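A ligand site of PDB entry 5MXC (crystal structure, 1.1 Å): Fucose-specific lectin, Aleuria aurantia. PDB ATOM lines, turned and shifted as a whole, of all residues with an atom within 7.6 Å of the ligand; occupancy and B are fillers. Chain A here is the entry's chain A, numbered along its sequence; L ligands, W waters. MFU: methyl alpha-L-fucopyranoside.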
ATOM      1  N   ILE A  14     -38.357  19.768 -22.098  1.00  0.00           N
ATOM      2  CA  ILE A  14     -38.388  20.774 -23.153  1.00  0.00           C
ATOM      3  C   ILE A  14     -38.299  20.110 -24.513  1.00  0.00           C
ATOM      4  O   ILE A  14     -37.877  18.954 -24.641  1.00  0.00           O
ATOM      5  CB  ILE A  14     -37.240  21.808 -22.980  1.00  0.00           C
ATOM      6  CG1 ILE A  14     -35.881  21.096 -22.967  1.00  0.00           C
ATOM      7  CG2 ILE A  14     -37.444  22.668 -21.731  1.00  0.00           C
ATOM      8  CD1 ILE A  14     -34.686  22.007 -22.977  1.00  0.00           C
ATOM      9  N   TRP A  16     -37.835  21.346 -28.976  1.00  0.00           N
ATOM     10  CA  TRP A  16     -37.805  22.361 -30.031  1.00  0.00           C
ATOM     11  C   TRP A  16     -37.700  21.714 -31.389  1.00  0.00           C
ATOM     12  O   TRP A  16     -37.156  20.617 -31.541  1.00  0.00           O
ATOM     13  CB  TRP A  16     -36.678  23.371 -29.800  1.00  0.00           C
ATOM     14  CG  TRP A  16     -35.254  22.836 -29.841  1.00  0.00           C
ATOM     15  CD1 TRP A  16     -34.390  22.880 -30.917  1.00  0.00           C
ATOM     16  CD2 TRP A  16     -34.509  22.257 -28.759  1.00  0.00           C
ATOM     17  NE1 TRP A  16     -33.191  22.338 -30.566  1.00  0.00           N
ATOM     18  CE2 TRP A  16     -33.230  21.960 -29.251  1.00  0.00           C
ATOM     19  CE3 TRP A  16     -34.810  21.952 -27.423  1.00  0.00           C
ATOM     20  CZ2 TRP A  16     -32.250  21.345 -28.456  1.00  0.00           C
ATOM     21  CZ3 TRP A  16     -33.844  21.353 -26.641  1.00  0.00           C
ATOM     22  CH2 TRP A  16     -32.565  21.065 -27.153  1.00  0.00           C
ATOM     23  N   GLN A  23     -35.941  18.037 -31.304  1.00  0.00           N
ATOM     24  CA  GLN A  23     -35.010  17.775 -30.189  1.00  0.00           C
ATOM     25  C   GLN A  23     -35.794  17.868 -28.882  1.00  0.00           C
ATOM     26  O   GLN A  23     -36.525  18.834 -28.665  1.00  0.00           O
ATOM     27  CB  GLN A  23     -33.871  18.784 -30.189  1.00  0.00           C
ATOM     28  CG  GLN A  23     -32.893  18.586 -31.344  1.00  0.00           C
ATOM     29  CD  GLN A  23     -32.042  17.336 -31.195  1.00  0.00           C
ATOM     30  OE1 GLN A  23     -31.683  16.939 -30.083  1.00  0.00           O
ATOM     31  NE2 GLN A  23     -31.710  16.706 -32.317  1.00  0.00           N
ATOM     32  N   GLN A  24     -35.597  16.862 -28.016  1.00  0.00           N
ATOM     33  CA  GLN A  24     -36.191  16.883 -26.669  1.00  0.00           C
ATOM     34  C   GLN A  24     -35.103  16.731 -25.644  1.00  0.00           C
ATOM     35  O   GLN A  24     -34.100  16.034 -25.866  1.00  0.00           O
ATOM     36  CB  GLN A  24     -37.171  15.739 -26.491  1.00  0.00           C
ATOM     37  CG  GLN A  24     -38.380  15.786 -27.390  1.00  0.00           C
ATOM     38  CD  GLN A  24     -39.298  14.627 -27.091  1.00  0.00           C
ATOM     39  OE1 GLN A  24     -40.015  14.626 -26.096  1.00  0.00           O
ATOM     40  NE2 GLN A  24     -39.255  13.613 -27.957  1.00  0.00           N
ATOM     41  N   ARG A  25     -35.298  17.387 -24.502  1.00  0.00           N
ATOM     42  CA  ARG A  25     -34.470  17.117 -23.312  1.00  0.00           C
ATOM     43  C   ARG A  25     -35.405  16.898 -22.143  1.00  0.00           C
ATOM     44  O   ARG A  25     -36.425  17.584 -22.004  1.00  0.00           O
ATOM     45  CB  ARG A  25     -33.521  18.274 -23.009  1.00  0.00           C
ATOM     46  CG  ARG A  25     -32.628  18.702 -24.158  1.00  0.00           C
ATOM     47  CD  ARG A  25     -31.554  17.684 -24.485  1.00  0.00           C
ATOM     48  NE  ARG A  25     -30.668  18.136 -25.564  1.00  0.00           N
ATOM     49  CZ  ARG A  25     -30.873  17.939 -26.865  1.00  0.00           C
ATOM     50  NH1 ARG A  25     -31.925  17.267 -27.303  1.00  0.00           N
ATOM     51  NH2 ARG A  25     -30.008  18.429 -27.746  1.00  0.00           N
ATOM     52  N   TYR A  27     -35.214  16.252 -17.775  1.00  0.00           N
ATOM     53  CA  TYR A  27     -34.411  16.428 -16.576  1.00  0.00           C
ATOM     54  C   TYR A  27     -35.065  15.700 -15.417  1.00  0.00           C
ATOM     55  O   TYR A  27     -36.294  15.760 -15.237  1.00  0.00           O
ATOM     56  CB  TYR A  27     -34.248  17.940 -16.235  1.00  0.00           C
ATOM     57  CG  TYR A  27     -33.612  18.653 -17.387  1.00  0.00           C
ATOM     58  CD1 TYR A  27     -32.241  18.595 -17.596  1.00  0.00           C
ATOM     59  CD2 TYR A  27     -34.395  19.291 -18.344  1.00  0.00           C
ATOM     60  CE1 TYR A  27     -31.665  19.163 -18.723  1.00  0.00           C
ATOM     61  CE2 TYR A  27     -33.828  19.855 -19.473  1.00  0.00           C
ATOM     62  CZ  TYR A  27     -32.471  19.773 -19.674  1.00  0.00           C
ATOM     63  OH  TYR A  27     -31.939  20.293 -20.827  1.00  0.00           O
ATOM     64  N   GLU A  37     -29.689  14.815 -17.451  1.00  0.00           N
ATOM     65  CA  GLU A  37     -30.384  15.071 -18.712  1.00  0.00           C
ATOM     66  C   GLU A  37     -30.390  13.819 -19.570  1.00  0.00           C
ATOM     67  O   GLU A  37     -29.367  13.137 -19.668  1.00  0.00           O
ATOM     68  CB  GLU A  37     -29.662  16.186 -19.474  1.00  0.00           C
ATOM     69  CG  GLU A  37     -30.357  16.686 -20.719  1.00  0.00           C
ATOM     70  CD  GLU A  37     -29.477  17.630 -21.515  1.00  0.00           C
ATOM     71  OE1 GLU A  37     -28.459  17.149 -22.052  1.00  0.00           O
ATOM     72  OE2 GLU A  37     -29.815  18.829 -21.627  1.00  0.00           O
ATOM     73  N   ALA A  38     -31.520  13.560 -20.219  1.00  0.00           N
ATOM     74  CA  ALA A  38     -31.607  12.623 -21.338  1.00  0.00           C
ATOM     75  C   ALA A  38     -32.050  13.417 -22.581  1.00  0.00           C
ATOM     76  O   ALA A  38     -32.730  14.457 -22.458  1.00  0.00           O
ATOM     77  CB  ALA A  38     -32.562  11.484 -21.045  1.00  0.00           C
ATOM     78  N   GLN A  39     -31.642  12.934 -23.766  1.00  0.00           N
ATOM     79  CA  GLN A  39     -31.842  13.648 -25.032  1.00  0.00           C
ATOM     80  C   GLN A  39     -32.490  12.754 -26.053  1.00  0.00           C
ATOM     81  O   GLN A  39     -32.224  11.551 -26.103  1.00  0.00           O
ATOM     82  CB  GLN A  39     -30.496  14.128 -25.598  1.00  0.00           C
ATOM     83  CG  GLN A  39     -29.557  14.810 -24.621  1.00  0.00           C
ATOM     84  CD  GLN A  39     -28.709  13.847 -23.789  1.00  0.00           C
ATOM     85  OE1 GLN A  39     -28.491  12.670 -24.161  1.00  0.00           O
ATOM     86  NE2 GLN A  39     -28.226  14.335 -22.664  1.00  0.00           N
ATOM     87  N   THR A  47     -30.970   9.060 -25.679  1.00  0.00           N
ATOM     88  CA  THR A  47     -29.615   8.961 -25.162  1.00  0.00           C
ATOM     89  C   THR A  47     -29.543   9.615 -23.787  1.00  0.00           C
ATOM     90  O   THR A  47     -30.490  10.263 -23.323  1.00  0.00           O
ATOM     91  CB  THR A  47     -28.634   9.652 -26.130  1.00  0.00           C
ATOM     92  OG1 THR A  47     -28.988  11.022 -26.308  1.00  0.00           O
ATOM     93  CG2 THR A  47     -28.637   8.980 -27.494  1.00  0.00           C
ATOM     94  N   ASN A  53     -24.149  12.469 -17.533  1.00  0.00           N
ATOM     95  CA  ASN A  53     -25.100  13.450 -18.057  1.00  0.00           C
ATOM     96  C   ASN A  53     -25.633  14.371 -16.959  1.00  0.00           C
ATOM     97  O   ASN A  53     -26.780  14.822 -17.017  1.00  0.00           O
ATOM     98  CB  ASN A  53     -26.241  12.701 -18.729  1.00  0.00           C
ATOM     99  CG  ASN A  53     -25.764  11.842 -19.876  1.00  0.00           C
ATOM    100  OD1 ASN A  53     -25.789  10.626 -19.797  1.00  0.00           O
ATOM    101  ND2 ASN A  53     -25.325  12.484 -20.965  1.00  0.00           N
ATOM    102  N   VAL A  54     -24.792  14.682 -15.980  1.00  0.00           N
ATOM    103  CA  VAL A  54     -25.166  15.581 -14.899  1.00  0.00           C
ATOM    104  C   VAL A  54     -25.045  17.024 -15.372  1.00  0.00           C
ATOM    105  O   VAL A  54     -24.021  17.419 -15.945  1.00  0.00           O
ATOM    106  CB  VAL A  54     -24.296  15.319 -13.652  1.00  0.00           C
ATOM    107  CG1 VAL A  54     -24.456  16.413 -12.604  1.00  0.00           C
ATOM    108  CG2 VAL A  54     -24.615  13.944 -13.079  1.00  0.00           C
ATOM    109  N   ILE A  55     -26.096  17.822 -15.139  1.00  0.00           N
ATOM    110  CA  ILE A  55     -26.139  19.239 -15.514  1.00  0.00           C
ATOM    111  C   ILE A  55     -26.169  20.165 -14.302  1.00  0.00           C
ATOM    112  O   ILE A  55     -26.014  21.377 -14.462  1.00  0.00           O
ATOM    113  CB  ILE A  55     -27.311  19.525 -16.493  1.00  0.00           C
ATOM    114  CG1 ILE A  55     -28.711  19.391 -15.850  1.00  0.00           C
ATOM    115  CG2 ILE A  55     -27.172  18.633 -17.731  1.00  0.00           C
ATOM    116  CD1 ILE A  55     -29.216  20.594 -15.098  1.00  0.00           C
ATOM    117  N   THR A  68     -36.570  26.712 -22.685  1.00  0.00           N
ATOM    118  CA  THR A  68     -35.557  26.807 -23.739  1.00  0.00           C
ATOM    119  C   THR A  68     -35.961  27.816 -24.798  1.00  0.00           C
ATOM    120  O   THR A  68     -37.143  28.065 -25.019  1.00  0.00           O
ATOM    121  CB  THR A  68     -35.302  25.404 -24.353  1.00  0.00           C
ATOM    122  OG1 THR A  68     -34.193  25.435 -25.250  1.00  0.00           O
ATOM    123  CG2 THR A  68     -36.497  24.894 -25.139  1.00  0.00           C
ATOM    124  N   GLY A  74     -26.501  29.980 -29.463  1.00  0.00           N
ATOM    125  CA  GLY A  74     -26.929  28.586 -29.573  1.00  0.00           C
ATOM    126  C   GLY A  74     -28.185  28.341 -28.775  1.00  0.00           C
ATOM    127  O   GLY A  74     -28.914  29.265 -28.405  1.00  0.00           O
ATOM    128  N   ILE A  75     -28.463  27.074 -28.520  1.00  0.00           N
ATOM    129  CA  ILE A  75     -29.635  26.687 -27.748  1.00  0.00           C
ATOM    130  C   ILE A  75     -29.405  27.092 -26.295  1.00  0.00           C
ATOM    131  O   ILE A  75     -28.384  26.752 -25.702  1.00  0.00           O
ATOM    132  CB  ILE A  75     -29.891  25.161 -27.850  1.00  0.00           C
ATOM    133  CG1 ILE A  75     -30.122  24.732 -29.322  1.00  0.00           C
ATOM    134  CG2 ILE A  75     -31.052  24.744 -26.943  1.00  0.00           C
ATOM    135  CD1 ILE A  75     -31.296  25.375 -30.014  1.00  0.00           C
ATOM    136  N   GLN A  76     -30.353  27.871 -25.763  1.00  0.00           N
ATOM    137  CA  GLN A  76     -30.341  28.244 -24.352  1.00  0.00           C
ATOM    138  C   GLN A  76     -31.310  27.353 -23.580  1.00  0.00           C
ATOM    139  O   GLN A  76     -32.440  27.130 -24.018  1.00  0.00           O
ATOM    140  CB  GLN A  76     -30.727  29.712 -24.163  1.00  0.00           C
ATOM    141  CG  GLN A  76     -29.809  30.717 -24.853  1.00  0.00           C
ATOM    142  CD  GLN A  76     -28.523  31.012 -24.110  1.00  0.00           C
ATOM    143  OE1 GLN A  76     -28.409  30.857 -22.897  1.00  0.00           O
ATOM    144  NE2 GLN A  76     -27.528  31.502 -24.850  1.00  0.00           N
ATOM    145  N   ILE A  77     -30.858  26.829 -22.442  1.00  0.00           N
ATOM    146  CA  ILE A  77     -31.725  26.055 -21.546  1.00  0.00           C
ATOM    147  C   ILE A  77     -31.567  26.634 -20.147  1.00  0.00           C
ATOM    148  O   ILE A  77     -30.460  27.004 -19.756  1.00  0.00           O
ATOM    149  CB  ILE A  77     -31.412  24.534 -21.543  1.00  0.00           C
ATOM    150  CG1 ILE A  77     -31.421  23.970 -22.970  1.00  0.00           C
ATOM    151  CG2 ILE A  77     -32.385  23.788 -20.643  1.00  0.00           C
ATOM    152  CD1 ILE A  77     -30.800  22.605 -23.106  1.00  0.00           C
ATOM    153  N   TYR A  93     -27.672  26.257 -19.590  1.00  0.00           N
ATOM    154  CA  TYR A  93     -26.925  25.812 -20.775  1.00  0.00           C
ATOM    155  C   TYR A  93     -26.878  27.046 -21.650  1.00  0.00           C
ATOM    156  O   TYR A  93     -27.928  27.557 -22.079  1.00  0.00           O
ATOM    157  CB  TYR A  93     -27.588  24.648 -21.500  1.00  0.00           C
ATOM    158  CG  TYR A  93     -26.739  24.134 -22.639  1.00  0.00           C
ATOM    159  CD1 TYR A  93     -25.622  23.347 -22.397  1.00  0.00           C
ATOM    160  CD2 TYR A  93     -27.033  24.487 -23.953  1.00  0.00           C
ATOM    161  CE1 TYR A  93     -24.824  22.886 -23.453  1.00  0.00           C
ATOM    162  CE2 TYR A  93     -26.239  24.034 -25.009  1.00  0.00           C
ATOM    163  CZ  TYR A  93     -25.149  23.229 -24.752  1.00  0.00           C
ATOM    164  OH  TYR A  93     -24.375  22.771 -25.801  1.00  0.00           O
ATOM    165  N   GLY A  95     -25.587  27.663 -24.613  1.00  0.00           N
ATOM    166  CA  GLY A  95     -25.311  27.416 -26.034  1.00  0.00           C
ATOM    167  C   GLY A  95     -24.137  26.501 -26.257  1.00  0.00           C
ATOM    168  O   GLY A  95     -24.042  25.881 -27.314  1.00  0.00           O
ATOM    169  N   SER A  96     -23.246  26.408 -25.263  1.00  0.00           N
ATOM    170  CA  SER A  96     -22.104  25.511 -25.380  1.00  0.00           C
ATOM    171  C   SER A  96     -21.762  24.727 -24.122  1.00  0.00           C
ATOM    172  O   SER A  96     -21.189  23.652 -24.240  1.00  0.00           O
ATOM    173  CB  SER A  96     -20.879  26.260 -25.888  1.00  0.00           C
ATOM    174  OG  SER A  96     -20.549  27.304 -25.009  1.00  0.00           O
ATOM    175  N   LYS A  97     -22.139  25.210 -22.933  1.00  0.00           N
ATOM    176  CA  LYS A  97     -21.803  24.517 -21.697  1.00  0.00           C
ATOM    177  C   LYS A  97     -22.826  24.780 -20.611  1.00  0.00           C
ATOM    178  O   LYS A  97     -23.587  25.760 -20.671  1.00  0.00           O
ATOM    179  CB  LYS A  97     -20.428  24.994 -21.197  1.00  0.00           C
ATOM    180  CG  LYS A  97     -20.373  26.485 -20.943  1.00  0.00           C
ATOM    181  CD  LYS A  97     -18.981  26.991 -20.552  1.00  0.00           C
ATOM    182  CE  LYS A  97     -18.980  28.508 -20.438  1.00  0.00           C
ATOM    183  NZ  LYS A  97     -19.286  29.197 -21.719  1.00  0.00           N
ATOM    184  N   TRP A  98     -22.805  23.916 -19.601  1.00  0.00           N
ATOM    185  CA  TRP A  98     -23.631  24.061 -18.412  1.00  0.00           C
ATOM    186  C   TRP A  98     -22.873  24.786 -17.311  1.00  0.00           C
ATOM    187  O   TRP A  98     -21.738  24.380 -16.983  1.00  0.00           O
ATOM    188  CB  TRP A  98     -24.051  22.668 -17.914  1.00  0.00           C
ATOM    189  CG  TRP A  98     -25.097  22.024 -18.756  1.00  0.00           C
ATOM    190  CD1 TRP A  98     -24.917  21.089 -19.734  1.00  0.00           C
ATOM    191  CD2 TRP A  98     -26.500  22.272 -18.697  1.00  0.00           C
ATOM    192  NE1 TRP A  98     -26.126  20.738 -20.282  1.00  0.00           N
ATOM    193  CE2 TRP A  98     -27.117  21.454 -19.674  1.00  0.00           C
ATOM    194  CE3 TRP A  98     -27.313  23.112 -17.913  1.00  0.00           C
ATOM    195  CZ2 TRP A  98     -28.490  21.432 -19.858  1.00  0.00           C
ATOM    196  CZ3 TRP A  98     -28.672  23.083 -18.105  1.00  0.00           C
ATOM    197  CH2 TRP A  98     -29.256  22.256 -19.067  1.00  0.00           C
HETATM  198  C1  MFU L   1     -26.581  18.631 -26.329  1.00  0.00           C
HETATM  199  C2  MFU L   1     -26.570  18.173 -24.873  1.00  0.00           C
HETATM  200  C3  MFU L   1     -26.532  19.389 -23.928  1.00  0.00           C
HETATM  201  C4  MFU L   1     -27.664  20.354 -24.266  1.00  0.00           C
HETATM  202  C5  MFU L   1     -27.573  20.739 -25.736  1.00  0.00           C
HETATM  203  C6  MFU L   1     -28.689  21.648 -26.202  1.00  0.00           C
HETATM  204  O1  MFU L   1     -25.319  19.239 -26.617  1.00  0.00           O
HETATM  205  O2  MFU L   1     -25.413  17.336 -24.645  1.00  0.00           O
HETATM  206  O3  MFU L   1     -26.578  18.948 -22.562  1.00  0.00           O
HETATM  207  O4  MFU L   1     -28.935  19.738 -24.050  1.00  0.00           O
HETATM  208  O5  MFU L   1     -27.653  19.551 -26.535  1.00  0.00           O
HETATM  209  CM  MFU L   1     -25.062  19.388 -28.017  1.00  0.00           C
HETATM  210  O   HOH W   1     -22.895  17.980 -25.373  1.00  0.00           O
HETATM  211  O   HOH W   2     -24.904  14.939 -23.555  1.00  0.00           O
HETATM  212  O   HOH W   3     -25.842  22.684 -28.374  1.00  0.00           O
HETATM  213  O   HOH W   4     -22.658  20.773 -25.165  1.00  0.00           O
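OE1 of Glu 37 is in hydrogen-bond range of O3 of the ligand (2.7 Å).
O4 of the ligand sits at hydrogen-bond distance from NE of Arg 25, 2.8 Å away.
An oxygen (O3) of the ligand is in hydrogen-bond range of the indole nitrogen (NE1) of Trp 98 (2.9 Å).
The side-chain carboxylate (OE1) of Glu 37 sits at hydrogen-bond distance from the side-chain amide nitrogen (NE2) of Gln 39.
The backbone NH (N) of Glu 37 lies within hydrogen-bond range of the backbone carbonyl oxygen (O) of Asn 53 (2.9 Å).
The guanidinium group (NH1) of Arg 25 sits at hydrogen-bond distance from the side-chain amide oxygen (OE1) of Gln 23 (2.8 Å).
The backbone carbonyl oxygen of Arg 25 lies within hydrogen-bond range of the backbone NH of Ile 14 (2.9 Å).
The backbone carbonyl oxygen of Ile 77 sits at hydrogen-bond distance from the backbone NH of Tyr 93, 2.9 Å away.
The side-chain hydroxyl of Tyr 93 lies within hydrogen-bond range of the backbone carbonyl oxygen of Gly 95, 3.5 Å away.
O of Tyr 93 sits close to OE1 of Gln 76 (3.4 Å).
The backbone carbonyl oxygen of Ile 75 is in hydrogen-bond range of the backbone NH of Gly 95, 3.1 Å away.
CG2 of Ile 75 touches C6 of the ligand (3.96 Å).
Ile 77 touches the ligand (CD1 to O4, 3.5 Å).
Tyr 93 touches the ligand.
Hydrophobic or aromatic side chains within 4 Å of the ligand: Ile 75, Ile 77, Tyr 93 and Trp 98.
The nearest printed residue that does not touch the ligand is Trp 16 (4.03 Å).
Water W2 lies within hydrogen-bond range of O2 of the ligand (2.7 Å) and NE2 of Gln 39 (3.5 Å).
Water W4 lies within hydrogen-bond range of the side-chain hydroxyl (OH) of Tyr 93 (2.7 Å), the backbone carbonyl oxygen (O) of Ser 96 (3.4 Å) and an oxygen (O1) of the ligand (3.4 Å).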
